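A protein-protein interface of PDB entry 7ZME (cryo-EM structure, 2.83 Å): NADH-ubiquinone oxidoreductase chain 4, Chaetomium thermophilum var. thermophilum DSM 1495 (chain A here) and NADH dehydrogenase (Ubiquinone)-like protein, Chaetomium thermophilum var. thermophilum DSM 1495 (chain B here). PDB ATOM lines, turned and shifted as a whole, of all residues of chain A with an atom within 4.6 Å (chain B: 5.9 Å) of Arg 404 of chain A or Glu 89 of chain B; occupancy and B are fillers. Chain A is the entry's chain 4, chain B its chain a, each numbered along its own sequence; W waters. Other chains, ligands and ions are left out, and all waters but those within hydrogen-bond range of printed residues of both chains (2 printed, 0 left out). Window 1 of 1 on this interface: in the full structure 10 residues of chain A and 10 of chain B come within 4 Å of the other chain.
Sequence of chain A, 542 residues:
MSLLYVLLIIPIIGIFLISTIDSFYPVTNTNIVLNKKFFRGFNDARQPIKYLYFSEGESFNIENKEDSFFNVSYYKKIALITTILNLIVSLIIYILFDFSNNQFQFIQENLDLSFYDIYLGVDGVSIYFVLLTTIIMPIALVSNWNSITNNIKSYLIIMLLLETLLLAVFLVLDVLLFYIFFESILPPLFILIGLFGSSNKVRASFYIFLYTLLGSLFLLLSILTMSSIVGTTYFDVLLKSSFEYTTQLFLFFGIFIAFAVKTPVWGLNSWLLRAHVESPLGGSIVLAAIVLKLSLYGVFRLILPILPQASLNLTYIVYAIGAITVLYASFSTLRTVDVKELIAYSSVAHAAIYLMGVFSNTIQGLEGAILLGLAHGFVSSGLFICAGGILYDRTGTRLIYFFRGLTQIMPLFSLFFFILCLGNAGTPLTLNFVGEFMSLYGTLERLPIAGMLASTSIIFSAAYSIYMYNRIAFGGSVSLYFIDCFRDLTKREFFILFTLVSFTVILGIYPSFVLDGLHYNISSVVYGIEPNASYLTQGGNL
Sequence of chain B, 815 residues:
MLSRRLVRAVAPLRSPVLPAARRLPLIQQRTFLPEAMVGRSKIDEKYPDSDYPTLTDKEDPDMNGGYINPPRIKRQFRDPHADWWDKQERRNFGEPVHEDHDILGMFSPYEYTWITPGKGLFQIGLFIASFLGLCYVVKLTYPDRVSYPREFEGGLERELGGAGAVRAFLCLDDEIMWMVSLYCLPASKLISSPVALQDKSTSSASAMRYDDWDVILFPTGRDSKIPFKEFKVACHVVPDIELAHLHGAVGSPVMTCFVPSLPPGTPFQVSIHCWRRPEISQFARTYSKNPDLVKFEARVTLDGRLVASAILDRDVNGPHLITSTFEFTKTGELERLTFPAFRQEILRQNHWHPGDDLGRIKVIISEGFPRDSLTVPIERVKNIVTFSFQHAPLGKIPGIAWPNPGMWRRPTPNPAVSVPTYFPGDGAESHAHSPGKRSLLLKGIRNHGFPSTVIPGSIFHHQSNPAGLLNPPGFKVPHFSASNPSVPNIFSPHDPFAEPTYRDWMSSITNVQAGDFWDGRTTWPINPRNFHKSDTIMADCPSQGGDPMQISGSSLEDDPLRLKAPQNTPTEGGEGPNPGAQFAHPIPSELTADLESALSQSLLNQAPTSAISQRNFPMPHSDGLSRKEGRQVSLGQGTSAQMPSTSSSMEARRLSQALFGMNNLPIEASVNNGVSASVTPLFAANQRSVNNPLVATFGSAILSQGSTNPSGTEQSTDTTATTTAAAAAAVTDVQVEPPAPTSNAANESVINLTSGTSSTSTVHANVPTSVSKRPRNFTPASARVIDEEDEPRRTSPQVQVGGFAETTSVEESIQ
Arg 404 of chain A touches Gln 88 of chain B (CZ to OE1, 3.7 Å). Arg 404 of chain A touches Glu 89 of chain B (NH1 to CG, 3.6 Å). Arg 471 of chain A touches Phe 107 of chain B. Gly 476 of chain A touches Gln 88 of chain B (CA to OE1, 3.2 Å). Asp 86 of chain B touches Leu 480 of chain A.
The guanidinium group (NH1) of Arg 404 of chain A lies within salt-bridge range of the side-chain carboxylate (OD2) of Asp 86 of chain B. N of Ser 477 of chain A is in hydrogen-bond range of OE1 of Gln 88 of chain B (3.1 Å).
Water W2 lies within hydrogen-bond range of OE2 of Glu 89 of chain B (2.6 Å), O of Gly 475 of chain A (3.0 Å) and NH1 of Arg 404 of chain A (3.4 Å). Water W1 lies within hydrogen-bond range of the side-chain carboxylate of Asp 86 of chain B (2.7 Å), the backbone NH of Leu 480 of chain A (2.7 Å) and the guanidinium group of Arg 404 of chain A (3.4 Å).
Hydrophobic or aromatic side chains of chain A that line the printed part of chain B: Leu 480. Among the printed residues, 7 pairs touch across the chains.
Printed residues of chain B within 4 Å of Arg 471 of chain A: Phe 107. Of the printed residues of chain B, Gly 476 of chain A touches Gln 88 (3.2 Å). Of the printed residues of chain B, Leu 480 of chain A touches Asp 86. Of the printed residues of chain A, Glu 89 of chain B touches Arg 404. Arg 90 of chain B touches none of the printed residues of chain A. Printed residues of chain A within 4 Å of Phe 107 of chain B: Arg 471 (3.7 Å). The nearest printed residue of chain B that does not touch Arg 404 of chain A is Lys 87 of chain B (6.5 Å). The nearest printed residue of chain A that does not touch Glu 89 of chain B is Gly 475 of chain A (4.9 Å). The nearest printed residue of chain B that does not touch Ser 477 of chain A is Asp 86 of chain B (7.0 Å).
NH2 of Arg 75 of chain B is in salt-bridge range of OE1 of Glu 89 of chain B (3.5 Å). OD1 of Asp 86 of chain B is in hydrogen-bond range of N of Glu 89 of chain B (3.5 Å). N of Asp 86 of chain B is in hydrogen-bond range of O of Arg 91 of chain B (3.0 Å). OE1 of Glu 89 of chain B lies within hydrogen-bond range of N of Met 106 of chain B (3.3 Å). O of Arg 404 of chain A lies within hydrogen-bond range of N of Ser 479 of chain A (2.9 Å). O of Ser 477 of chain A lies close to O of Gly 405 of chain A (2.7 Å).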
ATOM      1  N   PHE A 402     -15.516   1.490  -0.030  1.00  0.00           N
ATOM      2  CA  PHE A 402     -14.894   2.086   1.141  1.00  0.00           C
ATOM      3  C   PHE A 402     -15.581   3.359   1.614  1.00  0.00           C
ATOM      4  O   PHE A 402     -15.234   3.861   2.684  1.00  0.00           O
ATOM      5  CB  PHE A 402     -13.423   2.389   0.855  1.00  0.00           C
ATOM      6  CG  PHE A 402     -12.575   1.170   0.658  1.00  0.00           C
ATOM      7  CD1 PHE A 402     -12.102   0.461   1.741  1.00  0.00           C
ATOM      8  CD2 PHE A 402     -12.243   0.741  -0.614  1.00  0.00           C
ATOM      9  CE1 PHE A 402     -11.320  -0.657   1.562  1.00  0.00           C
ATOM     10  CE2 PHE A 402     -11.462  -0.378  -0.798  1.00  0.00           C
ATOM     11  CZ  PHE A 402     -10.999  -1.078   0.292  1.00  0.00           C
ATOM     12  N   PHE A 403     -16.529   3.900   0.857  1.00  0.00           N
ATOM     13  CA  PHE A 403     -17.173   5.158   1.201  1.00  0.00           C
ATOM     14  C   PHE A 403     -18.591   4.922   1.696  1.00  0.00           C
ATOM     15  O   PHE A 403     -19.315   4.064   1.183  1.00  0.00           O
ATOM     16  CB  PHE A 403     -17.215   6.116   0.011  1.00  0.00           C
ATOM     17  CG  PHE A 403     -15.867   6.494  -0.513  1.00  0.00           C
ATOM     18  CD1 PHE A 403     -15.184   5.658  -1.371  1.00  0.00           C
ATOM     19  CD2 PHE A 403     -15.286   7.691  -0.148  1.00  0.00           C
ATOM     20  CE1 PHE A 403     -13.950   6.004  -1.852  1.00  0.00           C
ATOM     21  CE2 PHE A 403     -14.050   8.042  -0.628  1.00  0.00           C
ATOM     22  CZ  PHE A 403     -13.381   7.196  -1.484  1.00  0.00           C
ATOM     23  N   ARG A 404     -18.978   5.710   2.699  1.00  0.00           N
ATOM     24  CA  ARG A 404     -20.309   5.650   3.283  1.00  0.00           C
ATOM     25  C   ARG A 404     -20.521   6.800   4.259  1.00  0.00           C
ATOM     26  O   ARG A 404     -19.614   7.142   5.022  1.00  0.00           O
ATOM     27  CB  ARG A 404     -20.509   4.317   3.997  1.00  0.00           C
ATOM     28  CG  ARG A 404     -21.891   4.118   4.554  1.00  0.00           C
ATOM     29  CD  ARG A 404     -21.942   2.861   5.372  1.00  0.00           C
ATOM     30  NE  ARG A 404     -21.242   3.015   6.638  1.00  0.00           N
ATOM     31  CZ  ARG A 404     -20.882   1.999   7.409  1.00  0.00           C
ATOM     32  NH1 ARG A 404     -21.149   0.758   7.033  1.00  0.00           N
ATOM     33  NH2 ARG A 404     -20.249   2.223   8.552  1.00  0.00           N
ATOM     34  N   GLY A 405     -21.706   7.401   4.237  1.00  0.00           N
ATOM     35  CA  GLY A 405     -22.090   8.366   5.256  1.00  0.00           C
ATOM     36  C   GLY A 405     -21.173   9.559   5.429  1.00  0.00           C
ATOM     37  O   GLY A 405     -20.933   9.987   6.562  1.00  0.00           O
ATOM     38  N   LEU A 406     -20.664  10.123   4.333  1.00  0.00           N
ATOM     39  CA  LEU A 406     -19.764  11.262   4.467  1.00  0.00           C
ATOM     40  C   LEU A 406     -20.479  12.553   4.831  1.00  0.00           C
ATOM     41  O   LEU A 406     -19.808  13.544   5.130  1.00  0.00           O
ATOM     42  CB  LEU A 406     -18.955  11.477   3.188  1.00  0.00           C
ATOM     43  CG  LEU A 406     -17.962  10.377   2.837  1.00  0.00           C
ATOM     44  CD1 LEU A 406     -17.337  10.649   1.495  1.00  0.00           C
ATOM     45  CD2 LEU A 406     -16.902  10.318   3.907  1.00  0.00           C
ATOM     46  N   ARG A 471     -25.023   6.120  -1.516  1.00  0.00           N
ATOM     47  CA  ARG A 471     -24.004   5.210  -1.020  1.00  0.00           C
ATOM     48  C   ARG A 471     -22.792   5.938  -0.460  1.00  0.00           C
ATOM     49  O   ARG A 471     -22.099   5.393   0.405  1.00  0.00           O
ATOM     50  CB  ARG A 471     -23.573   4.251  -2.129  1.00  0.00           C
ATOM     51  CG  ARG A 471     -24.483   3.048  -2.274  1.00  0.00           C
ATOM     52  CD  ARG A 471     -24.059   2.175  -3.434  1.00  0.00           C
ATOM     53  NE  ARG A 471     -24.043   2.919  -4.685  1.00  0.00           N
ATOM     54  CZ  ARG A 471     -23.508   2.474  -5.813  1.00  0.00           C
ATOM     55  NH1 ARG A 471     -22.941   1.281  -5.851  1.00  0.00           N
ATOM     56  NH2 ARG A 471     -23.537   3.222  -6.903  1.00  0.00           N
ATOM     57  N   ILE A 472     -22.529   7.158  -0.920  1.00  0.00           N
ATOM     58  CA  ILE A 472     -21.360   7.914  -0.483  1.00  0.00           C
ATOM     59  C   ILE A 472     -21.747   8.881   0.625  1.00  0.00           C
ATOM     60  O   ILE A 472     -21.184   8.841   1.723  1.00  0.00           O
ATOM     61  CB  ILE A 472     -20.713   8.657  -1.665  1.00  0.00           C
ATOM     62  CG1 ILE A 472     -20.250   7.659  -2.725  1.00  0.00           C
ATOM     63  CG2 ILE A 472     -19.558   9.524  -1.193  1.00  0.00           C
ATOM     64  CD1 ILE A 472     -19.769   8.295  -3.994  1.00  0.00           C
ATOM     65  N   PHE A 474     -24.804   9.238   2.100  1.00  0.00           N
ATOM     66  CA  PHE A 474     -25.805   8.677   2.996  1.00  0.00           C
ATOM     67  C   PHE A 474     -25.555   7.177   3.133  1.00  0.00           C
ATOM     68  O   PHE A 474     -24.506   6.663   2.745  1.00  0.00           O
ATOM     69  CB  PHE A 474     -27.224   8.936   2.481  1.00  0.00           C
ATOM     70  CG  PHE A 474     -27.653  10.374   2.509  1.00  0.00           C
ATOM     71  CD1 PHE A 474     -26.908  11.339   3.159  1.00  0.00           C
ATOM     72  CD2 PHE A 474     -28.822  10.757   1.877  1.00  0.00           C
ATOM     73  CE1 PHE A 474     -27.317  12.657   3.171  1.00  0.00           C
ATOM     74  CE2 PHE A 474     -29.234  12.072   1.890  1.00  0.00           C
ATOM     75  CZ  PHE A 474     -28.481  13.021   2.539  1.00  0.00           C
ATOM     76  N   GLY A 475     -26.524   6.477   3.712  1.00  0.00           N
ATOM     77  CA  GLY A 475     -26.490   5.030   3.757  1.00  0.00           C
ATOM     78  C   GLY A 475     -25.662   4.463   4.887  1.00  0.00           C
ATOM     79  O   GLY A 475     -24.979   3.451   4.717  1.00  0.00           O
ATOM     80  N   GLY A 476     -25.727   5.093   6.050  1.00  0.00           N
ATOM     81  CA  GLY A 476     -24.918   4.722   7.187  1.00  0.00           C
ATOM     82  C   GLY A 476     -24.347   5.940   7.872  1.00  0.00           C
ATOM     83  O   GLY A 476     -24.541   7.077   7.448  1.00  0.00           O
ATOM     84  N   SER A 477     -23.618   5.687   8.957  1.00  0.00           N
ATOM     85  CA  SER A 477     -23.116   6.805   9.752  1.00  0.00           C
ATOM     86  C   SER A 477     -21.859   7.395   9.122  1.00  0.00           C
ATOM     87  O   SER A 477     -21.879   8.515   8.607  1.00  0.00           O
ATOM     88  CB  SER A 477     -22.856   6.352  11.192  1.00  0.00           C
ATOM     89  OG  SER A 477     -21.896   5.314  11.243  1.00  0.00           O
ATOM     90  N   VAL A 478     -20.777   6.627   9.110  1.00  0.00           N
ATOM     91  CA  VAL A 478     -19.527   6.961   8.435  1.00  0.00           C
ATOM     92  C   VAL A 478     -18.850   5.639   8.124  1.00  0.00           C
ATOM     93  O   VAL A 478     -18.931   4.695   8.915  1.00  0.00           O
ATOM     94  CB  VAL A 478     -18.598   7.865   9.285  1.00  0.00           C
ATOM     95  CG1 VAL A 478     -17.209   7.932   8.679  1.00  0.00           C
ATOM     96  CG2 VAL A 478     -19.131   9.277   9.411  1.00  0.00           C
ATOM     97  N   SER A 479     -18.204   5.559   6.964  1.00  0.00           N
ATOM     98  CA  SER A 479     -17.525   4.330   6.580  1.00  0.00           C
ATOM     99  C   SER A 479     -16.510   3.930   7.644  1.00  0.00           C
ATOM    100  O   SER A 479     -15.719   4.753   8.108  1.00  0.00           O
ATOM    101  CB  SER A 479     -16.841   4.515   5.231  1.00  0.00           C
ATOM    102  OG  SER A 479     -16.146   3.348   4.842  1.00  0.00           O
ATOM    103  N   LEU A 480     -16.541   2.656   8.031  1.00  0.00           N
ATOM    104  CA  LEU A 480     -15.685   2.144   9.091  1.00  0.00           C
ATOM    105  C   LEU A 480     -14.290   1.788   8.604  1.00  0.00           C
ATOM    106  O   LEU A 480     -13.456   1.373   9.415  1.00  0.00           O
ATOM    107  CB  LEU A 480     -16.329   0.921   9.741  1.00  0.00           C
ATOM    108  CG  LEU A 480     -17.394   1.219  10.789  1.00  0.00           C
ATOM    109  CD1 LEU A 480     -17.888  -0.066  11.409  1.00  0.00           C
ATOM    110  CD2 LEU A 480     -16.841   2.152  11.852  1.00  0.00           C
ATOM    111  N   ARG B  75     -26.756 -10.039   2.158  1.00  0.00           N
ATOM    112  CA  ARG B  75     -26.254  -9.937   3.518  1.00  0.00           C
ATOM    113  C   ARG B  75     -27.365  -9.574   4.495  1.00  0.00           C
ATOM    114  O   ARG B  75     -27.115  -9.450   5.698  1.00  0.00           O
ATOM    115  CB  ARG B  75     -25.102  -8.932   3.551  1.00  0.00           C
ATOM    116  CG  ARG B  75     -24.168  -9.113   4.716  1.00  0.00           C
ATOM    117  CD  ARG B  75     -22.948  -8.228   4.599  1.00  0.00           C
ATOM    118  NE  ARG B  75     -22.223  -8.436   3.354  1.00  0.00           N
ATOM    119  CZ  ARG B  75     -22.000  -7.480   2.460  1.00  0.00           C
ATOM    120  NH1 ARG B  75     -21.340  -7.752   1.347  1.00  0.00           N
ATOM    121  NH2 ARG B  75     -22.417  -6.243   2.691  1.00  0.00           N
ATOM    122  N   ARG B  78     -27.782 -12.459   7.316  1.00  0.00           N
ATOM    123  CA  ARG B  78     -26.872 -12.712   8.416  1.00  0.00           C
ATOM    124  C   ARG B  78     -27.503 -12.271   9.734  1.00  0.00           C
ATOM    125  O   ARG B  78     -28.536 -11.602   9.770  1.00  0.00           O
ATOM    126  CB  ARG B  78     -25.547 -11.993   8.197  1.00  0.00           C
ATOM    127  CG  ARG B  78     -24.793 -12.448   6.973  1.00  0.00           C
ATOM    128  CD  ARG B  78     -23.409 -11.855   6.975  1.00  0.00           C
ATOM    129  NE  ARG B  78     -22.691 -12.098   5.733  1.00  0.00           N
ATOM    130  CZ  ARG B  78     -21.519 -11.547   5.447  1.00  0.00           C
ATOM    131  NH1 ARG B  78     -20.917 -11.811   4.296  1.00  0.00           N
ATOM    132  NH2 ARG B  78     -20.950 -10.727   6.318  1.00  0.00           N
ATOM    133  N   ASP B  86     -18.316  -4.380  11.060  1.00  0.00           N
ATOM    134  CA  ASP B  86     -19.244  -3.376  10.560  1.00  0.00           C
ATOM    135  C   ASP B  86     -20.641  -3.878  10.903  1.00  0.00           C
ATOM    136  O   ASP B  86     -21.213  -4.687  10.170  1.00  0.00           O
ATOM    137  CB  ASP B  86     -19.071  -3.171   9.059  1.00  0.00           C
ATOM    138  CG  ASP B  86     -19.589  -1.831   8.585  1.00  0.00           C
ATOM    139  OD1 ASP B  86     -20.428  -1.229   9.286  1.00  0.00           O
ATOM    140  OD2 ASP B  86     -19.160  -1.381   7.506  1.00  0.00           O
ATOM    141  N   LYS B  87     -21.179  -3.411  12.030  1.00  0.00           N
ATOM    142  CA  LYS B  87     -22.497  -3.866  12.457  1.00  0.00           C
ATOM    143  C   LYS B  87     -23.575  -3.447  11.466  1.00  0.00           C
ATOM    144  O   LYS B  87     -24.497  -4.216  11.177  1.00  0.00           O
ATOM    145  CB  LYS B  87     -22.811  -3.333  13.854  1.00  0.00           C
ATOM    146  CG  LYS B  87     -24.111  -3.864  14.434  1.00  0.00           C
ATOM    147  CD  LYS B  87     -24.404  -3.253  15.792  1.00  0.00           C
ATOM    148  CE  LYS B  87     -23.491  -3.826  16.862  1.00  0.00           C
ATOM    149  NZ  LYS B  87     -23.842  -3.325  18.218  1.00  0.00           N
ATOM    150  N   GLN B  88     -23.474  -2.225  10.937  1.00  0.00           N
ATOM    151  CA  GLN B  88     -24.450  -1.751   9.964  1.00  0.00           C
ATOM    152  C   GLN B  88     -24.445  -2.609   8.710  1.00  0.00           C
ATOM    153  O   GLN B  88     -25.505  -2.951   8.177  1.00  0.00           O
ATOM    154  CB  GLN B  88     -24.162  -0.297   9.603  1.00  0.00           C
ATOM    155  CG  GLN B  88     -24.985   0.713  10.364  1.00  0.00           C
ATOM    156  CD  GLN B  88     -25.019   2.042   9.662  1.00  0.00           C
ATOM    157  OE1 GLN B  88     -23.977   2.607   9.339  1.00  0.00           O
ATOM    158  NE2 GLN B  88     -26.217   2.548   9.409  1.00  0.00           N
ATOM    159  N   GLU B  89     -23.258  -2.963   8.223  1.00  0.00           N
ATOM    160  CA  GLU B  89     -23.162  -3.791   7.031  1.00  0.00           C
ATOM    161  C   GLU B  89     -23.283  -5.277   7.326  1.00  0.00           C
ATOM    162  O   GLU B  89     -23.600  -6.037   6.413  1.00  0.00           O
ATOM    163  CB  GLU B  89     -21.845  -3.514   6.308  1.00  0.00           C
ATOM    164  CG  GLU B  89     -21.919  -2.339   5.355  1.00  0.00           C
ATOM    165  CD  GLU B  89     -23.249  -2.269   4.636  1.00  0.00           C
ATOM    166  OE1 GLU B  89     -23.505  -3.135   3.778  1.00  0.00           O
ATOM    167  OE2 GLU B  89     -24.041  -1.351   4.932  1.00  0.00           O
ATOM    168  N   ARG B  90     -23.066  -5.695   8.576  1.00  0.00           N
ATOM    169  CA  ARG B  90     -23.072  -7.104   8.984  1.00  0.00           C
ATOM    170  C   ARG B  90     -21.953  -7.882   8.291  1.00  0.00           C
ATOM    171  O   ARG B  90     -22.177  -8.896   7.628  1.00  0.00           O
ATOM    172  CB  ARG B  90     -24.432  -7.759   8.724  1.00  0.00           C
ATOM    173  CG  ARG B  90     -25.609  -7.018   9.315  1.00  0.00           C
ATOM    174  CD  ARG B  90     -26.675  -7.988   9.741  1.00  0.00           C
ATOM    175  NE  ARG B  90     -27.940  -7.326  10.011  1.00  0.00           N
ATOM    176  CZ  ARG B  90     -29.100  -7.718   9.498  1.00  0.00           C
ATOM    177  NH1 ARG B  90     -29.147  -8.768   8.691  1.00  0.00           N
ATOM    178  NH2 ARG B  90     -30.211  -7.060   9.791  1.00  0.00           N
ATOM    179  N   ARG B  91     -20.728  -7.396   8.473  1.00  0.00           N
ATOM    180  CA  ARG B  91     -19.577  -7.965   7.794  1.00  0.00           C
ATOM    181  C   ARG B  91     -18.345  -7.828   8.680  1.00  0.00           C
ATOM    182  O   ARG B  91     -18.193  -6.845   9.409  1.00  0.00           O
ATOM    183  CB  ARG B  91     -19.348  -7.279   6.442  1.00  0.00           C
ATOM    184  CG  ARG B  91     -18.342  -7.971   5.556  1.00  0.00           C
ATOM    185  CD  ARG B  91     -17.907  -7.092   4.394  1.00  0.00           C
ATOM    186  NE  ARG B  91     -16.787  -7.695   3.678  1.00  0.00           N
ATOM    187  CZ  ARG B  91     -15.513  -7.380   3.883  1.00  0.00           C
ATOM    188  NH1 ARG B  91     -15.191  -6.457   4.776  1.00  0.00           N
ATOM    189  NH2 ARG B  91     -14.561  -7.988   3.192  1.00  0.00           N
ATOM    190  N   GLY B 105     -25.157  -6.257  -0.407  1.00  0.00           N
ATOM    191  CA  GLY B 105     -25.024  -5.689   0.916  1.00  0.00           C
ATOM    192  C   GLY B 105     -26.354  -5.281   1.516  1.00  0.00           C
ATOM    193  O   GLY B 105     -27.429  -5.549   0.979  1.00  0.00           O
ATOM    194  N   MET B 106     -26.265  -4.628   2.676  1.00  0.00           N
ATOM    195  CA  MET B 106     -27.476  -4.201   3.371  1.00  0.00           C
ATOM    196  C   MET B 106     -28.241  -3.155   2.570  1.00  0.00           C
ATOM    197  O   MET B 106     -29.475  -3.205   2.497  1.00  0.00           O
ATOM    198  CB  MET B 106     -27.131  -3.670   4.761  1.00  0.00           C
ATOM    199  CG  MET B 106     -26.619  -4.727   5.726  1.00  0.00           C
ATOM    200  SD  MET B 106     -27.644  -6.204   5.825  1.00  0.00           S
ATOM    201  CE  MET B 106     -29.192  -5.516   6.399  1.00  0.00           C
ATOM    202  N   PHE B 107     -27.515  -2.167   2.039  1.00  0.00           N
ATOM    203  CA  PHE B 107     -28.144  -1.125   1.190  1.00  0.00           C
ATOM    204  C   PHE B 107     -28.306  -1.689  -0.215  1.00  0.00           C
ATOM    205  O   PHE B 107     -27.507  -1.356  -1.101  1.00  0.00           O
ATOM    206  CB  PHE B 107     -27.326   0.161   1.166  1.00  0.00           C
ATOM    207  CG  PHE B 107     -27.994   1.314   0.457  1.00  0.00           C
ATOM    208  CD1 PHE B 107     -29.352   1.293   0.185  1.00  0.00           C
ATOM    209  CD2 PHE B 107     -27.265   2.422   0.063  1.00  0.00           C
ATOM    210  CE1 PHE B 107     -29.963   2.345  -0.474  1.00  0.00           C
ATOM    211  CE2 PHE B 107     -27.879   3.476  -0.589  1.00  0.00           C
ATOM    212  CZ  PHE B 107     -29.226   3.438  -0.857  1.00  0.00           C
HETATM  213  O   HOH W   1     -17.744   0.708   6.677  1.00  0.00           O
HETATM  214  O   HOH W   2     -24.405   0.906   6.143  1.00  0.00           O
